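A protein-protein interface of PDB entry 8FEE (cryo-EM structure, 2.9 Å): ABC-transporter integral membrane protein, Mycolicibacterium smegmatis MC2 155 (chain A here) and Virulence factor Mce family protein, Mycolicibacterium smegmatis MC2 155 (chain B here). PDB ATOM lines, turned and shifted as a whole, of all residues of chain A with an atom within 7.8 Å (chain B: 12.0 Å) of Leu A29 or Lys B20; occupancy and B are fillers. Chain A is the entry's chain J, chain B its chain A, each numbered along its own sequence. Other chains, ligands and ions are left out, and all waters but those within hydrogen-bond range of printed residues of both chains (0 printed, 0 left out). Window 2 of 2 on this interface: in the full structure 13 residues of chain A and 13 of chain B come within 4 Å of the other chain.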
ATOM      1  N   ARG A  27      12.622 -20.661 -26.303  1.00  0.00           N
ATOM      2  CA  ARG A  27      12.409 -20.355 -27.712  1.00  0.00           C
ATOM      3  C   ARG A  27      11.120 -20.985 -28.225  1.00  0.00           C
ATOM      4  O   ARG A  27      10.106 -20.303 -28.385  1.00  0.00           O
ATOM      5  CB  ARG A  27      13.597 -20.834 -28.547  1.00  0.00           C
ATOM      6  CG  ARG A  27      14.739 -19.837 -28.628  1.00  0.00           C
ATOM      7  CD  ARG A  27      14.276 -18.537 -29.264  1.00  0.00           C
ATOM      8  NE  ARG A  27      13.749 -18.754 -30.606  1.00  0.00           N
ATOM      9  CZ  ARG A  27      13.241 -17.800 -31.376  1.00  0.00           C
ATOM     10  NH1 ARG A  27      13.171 -16.545 -30.965  1.00  0.00           N
ATOM     11  NH2 ARG A  27      12.793 -18.116 -32.587  1.00  0.00           N
ATOM     12  N   PHE A  28      11.180 -22.291 -28.499  1.00  0.00           N
ATOM     13  CA  PHE A  28      10.008 -23.010 -28.991  1.00  0.00           C
ATOM     14  C   PHE A  28       8.873 -22.963 -27.976  1.00  0.00           C
ATOM     15  O   PHE A  28       7.723 -22.658 -28.321  1.00  0.00           O
ATOM     16  CB  PHE A  28      10.395 -24.455 -29.314  1.00  0.00           C
ATOM     17  CG  PHE A  28       9.287 -25.261 -29.926  1.00  0.00           C
ATOM     18  CD1 PHE A  28       8.979 -25.132 -31.271  1.00  0.00           C
ATOM     19  CD2 PHE A  28       8.566 -26.163 -29.161  1.00  0.00           C
ATOM     20  CE1 PHE A  28       7.963 -25.879 -31.837  1.00  0.00           C
ATOM     21  CE2 PHE A  28       7.551 -26.914 -29.722  1.00  0.00           C
ATOM     22  CZ  PHE A  28       7.249 -26.771 -31.062  1.00  0.00           C
ATOM     23  N   LEU A  29       9.188 -23.242 -26.709  1.00  0.00           N
ATOM     24  CA  LEU A  29       8.192 -23.135 -25.650  1.00  0.00           C
ATOM     25  C   LEU A  29       7.706 -21.700 -25.499  1.00  0.00           C
ATOM     26  O   LEU A  29       6.512 -21.462 -25.292  1.00  0.00           O
ATOM     27  CB  LEU A  29       8.758 -23.667 -24.332  1.00  0.00           C
ATOM     28  CG  LEU A  29       7.837 -23.572 -23.113  1.00  0.00           C
ATOM     29  CD1 LEU A  29       6.533 -24.306 -23.375  1.00  0.00           C
ATOM     30  CD2 LEU A  29       8.522 -24.146 -21.885  1.00  0.00           C
ATOM     31  N   ASP A  30       8.618 -20.728 -25.591  1.00  0.00           N
ATOM     32  CA  ASP A  30       8.213 -19.330 -25.491  1.00  0.00           C
ATOM     33  C   ASP A  30       7.339 -18.918 -26.674  1.00  0.00           C
ATOM     34  O   ASP A  30       6.392 -18.142 -26.509  1.00  0.00           O
ATOM     35  CB  ASP A  30       9.448 -18.433 -25.394  1.00  0.00           C
ATOM     36  CG  ASP A  30       9.136 -17.070 -24.804  1.00  0.00           C
ATOM     37  OD1 ASP A  30       7.973 -16.841 -24.409  1.00  0.00           O
ATOM     38  OD2 ASP A  30      10.056 -16.228 -24.734  1.00  0.00           O
ATOM     39  N   SER A  31       7.654 -19.408 -27.877  1.00  0.00           N
ATOM     40  CA  SER A  31       6.817 -19.121 -29.041  1.00  0.00           C
ATOM     41  C   SER A  31       5.418 -19.703 -28.873  1.00  0.00           C
ATOM     42  O   SER A  31       4.410 -19.039 -29.177  1.00  0.00           O
ATOM     43  CB  SER A  31       7.476 -19.665 -30.308  1.00  0.00           C
ATOM     44  OG  SER A  31       6.659 -19.437 -31.444  1.00  0.00           O
ATOM     45  N   MET A  32       5.335 -20.936 -28.358  1.00  0.00           N
ATOM     46  CA  MET A  32       4.028 -21.518 -28.078  1.00  0.00           C
ATOM     47  C   MET A  32       3.303 -20.718 -27.010  1.00  0.00           C
ATOM     48  O   MET A  32       2.081 -20.546 -27.080  1.00  0.00           O
ATOM     49  CB  MET A  32       4.172 -22.978 -27.646  1.00  0.00           C
ATOM     50  CG  MET A  32       4.771 -23.893 -28.697  1.00  0.00           C
ATOM     51  SD  MET A  32       4.675 -25.624 -28.203  1.00  0.00           S
ATOM     52  CE  MET A  32       2.911 -25.804 -27.950  1.00  0.00           C
ATOM     53  N   GLY A  33       4.029 -20.235 -26.003  1.00  0.00           N
ATOM     54  CA  GLY A  33       3.386 -19.436 -24.980  1.00  0.00           C
ATOM     55  C   GLY A  33       2.867 -18.128 -25.531  1.00  0.00           C
ATOM     56  O   GLY A  33       1.824 -17.638 -25.097  1.00  0.00           O
ATOM     57  N   HIS A  34       3.592 -17.544 -26.486  1.00  0.00           N
ATOM     58  CA  HIS A  34       3.163 -16.295 -27.104  1.00  0.00           C
ATOM     59  C   HIS A  34       1.862 -16.489 -27.873  1.00  0.00           C
ATOM     60  O   HIS A  34       0.912 -15.708 -27.723  1.00  0.00           O
ATOM     61  CB  HIS A  34       4.262 -15.759 -28.021  1.00  0.00           C
ATOM     62  CG  HIS A  34       4.065 -14.333 -28.431  1.00  0.00           C
ATOM     63  ND1 HIS A  34       3.493 -13.393 -27.602  1.00  0.00           N
ATOM     64  CD2 HIS A  34       4.368 -13.685 -29.581  1.00  0.00           C
ATOM     65  CE1 HIS A  34       3.449 -12.229 -28.224  1.00  0.00           C
ATOM     66  NE2 HIS A  34       3.974 -12.379 -29.426  1.00  0.00           N
ATOM     67  N   VAL A  35       1.794 -17.543 -28.693  1.00  0.00           N
ATOM     68  CA  VAL A  35       0.553 -17.765 -29.438  1.00  0.00           C
ATOM     69  C   VAL A  35      -0.577 -18.187 -28.498  1.00  0.00           C
ATOM     70  O   VAL A  35      -1.740 -17.821 -28.714  1.00  0.00           O
ATOM     71  CB  VAL A  35       0.766 -18.772 -30.590  1.00  0.00           C
ATOM     72  CG1 VAL A  35       1.481 -20.011 -30.119  1.00  0.00           C
ATOM     73  CG2 VAL A  35      -0.554 -19.132 -31.269  1.00  0.00           C
ATOM     74  N   ALA A  36      -0.262 -18.931 -27.432  1.00  0.00           N
ATOM     75  CA  ALA A  36      -1.269 -19.276 -26.433  1.00  0.00           C
ATOM     76  C   ALA A  36      -1.827 -18.033 -25.751  1.00  0.00           C
ATOM     77  O   ALA A  36      -3.043 -17.912 -25.560  1.00  0.00           O
ATOM     78  CB  ALA A  36      -0.675 -20.234 -25.402  1.00  0.00           C
ATOM     79  N   PRO B  18       3.928 -14.355 -18.149  1.00  0.00           N
ATOM     80  CA  PRO B  18       3.435 -15.724 -17.970  1.00  0.00           C
ATOM     81  C   PRO B  18       3.311 -16.473 -19.292  1.00  0.00           C
ATOM     82  O   PRO B  18       2.327 -17.180 -19.511  1.00  0.00           O
ATOM     83  CB  PRO B  18       2.062 -15.515 -17.332  1.00  0.00           C
ATOM     84  CG  PRO B  18       1.613 -14.200 -17.869  1.00  0.00           C
ATOM     85  CD  PRO B  18       2.857 -13.357 -17.972  1.00  0.00           C
ATOM     86  N   TYR B  19       4.304 -16.306 -20.167  1.00  0.00           N
ATOM     87  CA  TYR B  19       4.260 -16.957 -21.472  1.00  0.00           C
ATOM     88  C   TYR B  19       4.446 -18.465 -21.356  1.00  0.00           C
ATOM     89  O   TYR B  19       3.663 -19.237 -21.917  1.00  0.00           O
ATOM     90  CB  TYR B  19       5.317 -16.356 -22.402  1.00  0.00           C
ATOM     91  CG  TYR B  19       5.109 -14.893 -22.723  1.00  0.00           C
ATOM     92  CD1 TYR B  19       3.848 -14.315 -22.644  1.00  0.00           C
ATOM     93  CD2 TYR B  19       6.172 -14.093 -23.118  1.00  0.00           C
ATOM     94  CE1 TYR B  19       3.654 -12.980 -22.940  1.00  0.00           C
ATOM     95  CE2 TYR B  19       5.988 -12.756 -23.418  1.00  0.00           C
ATOM     96  CZ  TYR B  19       4.728 -12.205 -23.326  1.00  0.00           C
ATOM     97  OH  TYR B  19       4.540 -10.876 -23.624  1.00  0.00           O
ATOM     98  N   LYS B  20       5.463 -18.904 -20.609  1.00  0.00           N
ATOM     99  CA  LYS B  20       5.735 -20.335 -20.498  1.00  0.00           C
ATOM    100  C   LYS B  20       4.602 -21.083 -19.801  1.00  0.00           C
ATOM    101  O   LYS B  20       4.332 -22.246 -20.132  1.00  0.00           O
ATOM    102  CB  LYS B  20       7.050 -20.543 -19.747  1.00  0.00           C
ATOM    103  CG  LYS B  20       8.184 -19.655 -20.249  1.00  0.00           C
ATOM    104  CD  LYS B  20       9.502 -19.961 -19.552  1.00  0.00           C
ATOM    105  CE  LYS B  20      10.033 -21.331 -19.928  1.00  0.00           C
ATOM    106  NZ  LYS B  20      10.290 -21.416 -21.392  1.00  0.00           N
ATOM    107  N   LEU B  21       3.879 -20.407 -18.904  1.00  0.00           N
ATOM    108  CA  LEU B  21       2.721 -21.022 -18.262  1.00  0.00           C
ATOM    109  C   LEU B  21       1.621 -21.300 -19.280  1.00  0.00           C
ATOM    110  O   LEU B  21       1.059 -22.405 -19.316  1.00  0.00           O
ATOM    111  CB  LEU B  21       2.230 -20.113 -17.131  1.00  0.00           C
ATOM    112  CG  LEU B  21       1.242 -20.599 -16.066  1.00  0.00           C
ATOM    113  CD1 LEU B  21      -0.198 -20.460 -16.522  1.00  0.00           C
ATOM    114  CD2 LEU B  21       1.546 -22.038 -15.674  1.00  0.00           C
ATOM    115  N   ALA B  22       1.365 -20.348 -20.179  1.00  0.00           N
ATOM    116  CA  ALA B  22       0.303 -20.572 -21.148  1.00  0.00           C
ATOM    117  C   ALA B  22       0.764 -21.546 -22.216  1.00  0.00           C
ATOM    118  O   ALA B  22      -0.059 -22.263 -22.793  1.00  0.00           O
ATOM    119  CB  ALA B  22      -0.136 -19.249 -21.776  1.00  0.00           C
ATOM    120  N   GLY B  23       2.068 -21.569 -22.503  1.00  0.00           N
ATOM    121  CA  GLY B  23       2.582 -22.539 -23.451  1.00  0.00           C
ATOM    122  C   GLY B  23       2.388 -23.953 -22.943  1.00  0.00           C
ATOM    123  O   GLY B  23       1.992 -24.849 -23.694  1.00  0.00           O
ATOM    124  N   LEU B  24       2.663 -24.167 -21.649  1.00  0.00           N
ATOM    125  CA  LEU B  24       2.415 -25.471 -21.044  1.00  0.00           C
ATOM    126  C   LEU B  24       0.931 -25.813 -21.062  1.00  0.00           C
ATOM    127  O   LEU B  24       0.558 -26.966 -21.314  1.00  0.00           O
ATOM    128  CB  LEU B  24       2.959 -25.508 -19.617  1.00  0.00           C
ATOM    129  CG  LEU B  24       4.479 -25.420 -19.460  1.00  0.00           C
ATOM    130  CD1 LEU B  24       4.873 -25.500 -17.993  1.00  0.00           C
ATOM    131  CD2 LEU B  24       5.166 -26.513 -20.264  1.00  0.00           C
ATOM    132  N   ILE B  25       0.065 -24.824 -20.809  1.00  0.00           N
ATOM    133  CA  ILE B  25      -1.377 -25.082 -20.850  1.00  0.00           C
ATOM    134  C   ILE B  25      -1.813 -25.504 -22.250  1.00  0.00           C
ATOM    135  O   ILE B  25      -2.569 -26.467 -22.419  1.00  0.00           O
ATOM    136  CB  ILE B  25      -2.175 -23.860 -20.362  1.00  0.00           C
ATOM    137  CG1 ILE B  25      -1.846 -23.533 -18.908  1.00  0.00           C
ATOM    138  CG2 ILE B  25      -3.672 -24.093 -20.527  1.00  0.00           C
ATOM    139  CD1 ILE B  25      -2.623 -22.352 -18.376  1.00  0.00           C
ATOM    140  N   LEU B  26      -1.338 -24.791 -23.274  1.00  0.00           N
ATOM    141  CA  LEU B  26      -1.703 -25.124 -24.649  1.00  0.00           C
ATOM    142  C   LEU B  26      -1.176 -26.495 -25.053  1.00  0.00           C
ATOM    143  O   LEU B  26      -1.883 -27.269 -25.712  1.00  0.00           O
ATOM    144  CB  LEU B  26      -1.189 -24.046 -25.604  1.00  0.00           C
ATOM    145  CG  LEU B  26      -1.751 -24.086 -27.026  1.00  0.00           C
ATOM    146  CD1 LEU B  26      -3.246 -23.800 -27.019  1.00  0.00           C
ATOM    147  CD2 LEU B  26      -1.020 -23.101 -27.927  1.00  0.00           C
ATOM    148  N   GLY B  27       0.068 -26.810 -24.685  1.00  0.00           N
ATOM    149  CA  GLY B  27       0.603 -28.126 -24.993  1.00  0.00           C
ATOM    150  C   GLY B  27      -0.166 -29.241 -24.310  1.00  0.00           C
ATOM    151  O   GLY B  27      -0.430 -30.287 -24.914  1.00  0.00           O
ATOM    152  N   LEU B  28      -0.544 -29.030 -23.045  1.00  0.00           N
ATOM    153  CA  LEU B  28      -1.350 -30.019 -22.338  1.00  0.00           C
ATOM    154  C   LEU B  28      -2.718 -30.185 -22.985  1.00  0.00           C
ATOM    155  O   LEU B  28      -3.223 -31.307 -23.100  1.00  0.00           O
ATOM    156  CB  LEU B  28      -1.497 -29.621 -20.869  1.00  0.00           C
ATOM    157  CG  LEU B  28      -2.229 -30.624 -19.975  1.00  0.00           C
ATOM    158  CD1 LEU B  28      -1.429 -31.911 -19.850  1.00  0.00           C
ATOM    159  CD2 LEU B  28      -2.507 -30.023 -18.607  1.00  0.00           C
ATOM    160  N   VAL B  29      -3.334 -29.079 -23.412  1.00  0.00           N
ATOM    161  CA  VAL B  29      -4.621 -29.153 -24.102  1.00  0.00           C
ATOM    162  C   VAL B  29      -4.494 -29.959 -25.389  1.00  0.00           C
ATOM    163  O   VAL B  29      -5.333 -30.819 -25.684  1.00  0.00           O
ATOM    164  CB  VAL B  29      -5.170 -27.737 -24.367  1.00  0.00           C
ATOM    165  CG1 VAL B  29      -6.303 -27.780 -25.381  1.00  0.00           C
ATOM    166  CG2 VAL B  29      -5.654 -27.109 -23.072  1.00  0.00           C
ATOM    167  N   GLY B  30      -3.441 -29.701 -26.169  1.00  0.00           N
ATOM    168  CA  GLY B  30      -3.247 -30.448 -27.404  1.00  0.00           C
ATOM    169  C   GLY B  30      -3.038 -31.933 -27.167  1.00  0.00           C
ATOM    170  O   GLY B  30      -3.639 -32.776 -27.843  1.00  0.00           O
ATOM    171  N   VAL B  31      -2.184 -32.271 -26.195  1.00  0.00           N
ATOM    172  CA  VAL B  31      -1.915 -33.677 -25.898  1.00  0.00           C
ATOM    173  C   VAL B  31      -3.177 -34.369 -25.396  1.00  0.00           C
ATOM    174  O   VAL B  31      -3.470 -35.510 -25.776  1.00  0.00           O
ATOM    175  CB  VAL B  31      -0.756 -33.795 -24.887  1.00  0.00           C
ATOM    176  CG1 VAL B  31      -0.623 -35.223 -24.381  1.00  0.00           C
ATOM    177  CG2 VAL B  31       0.547 -33.338 -25.523  1.00  0.00           C
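Leu A29 touches Lys B20.
Tyr B19 touches Asp A30 (CB to OD1, 3.4 Å).
Gly A33 touches Tyr B19.
Gly B23 touches Gly A33 (N to CA, 3.5 Å).
Ala A36 touches Ala B22.
CB of Ala A36 touches CD2 of Leu B26 (3.8 Å).
Of the 14 printed residues of chain B, 5 touch a printed residue of chain A.
Printed residues of chain B that touch a printed residue of chain A: Tyr B19, Lys B20, Ala B22, Gly B23 and Leu B26.
Hydrophobic or aromatic side chains of chain B within 4 Å of the printed part of chain A: Tyr B19, Ala B22 and Leu B26.
Hydrophobic or aromatic side chains of chain A within 4 Å of the printed part of chain B: Leu A29 and Ala A36.
Among the printed residues, no Asp or Glu carboxylate lies within 4 Å of a Lys or Arg side-chain nitrogen of the other chain.
Of chain B, only Lys B20 (3.3 Å) comes within 4 Å of Leu A29.
Lys B20 touches just one residue of chain A: Leu A29 (3.3 Å).
No residue of chain B comes within 4 Å of Phe A28.
Asp A30 touches just one residue of chain B: Tyr B19 (3.4 Å).
No residue of chain B comes within 4 Å of Met A32.
Of the printed residues of chain B, Gly A33 touches Tyr B19 and Gly B23.
Of the printed residues of chain A, Ala B22 touches Ala A36.
Of the printed residues of chain B, Ala A36 touches Ala B22 (3.4 Å) and Leu B26 (3.8 Å).
Of the printed residues of chain A, Leu B26 touches Ala A36.
Of the printed residues of chain A, Gly B23 touches Gly A33 (3.5 Å).
Of the printed residues of chain A, Tyr B19 touches Asp A30 (3.4 Å) and Gly A33 (3.1 Å).
Leu B24 touches none of the printed residues of chain A.
The nearest residue of chain B that does not touch Leu A29 is Leu B24 (4.1 Å).
The nearest residue of chain A that does not touch Lys B20 is Asp A30 (4.6 Å).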
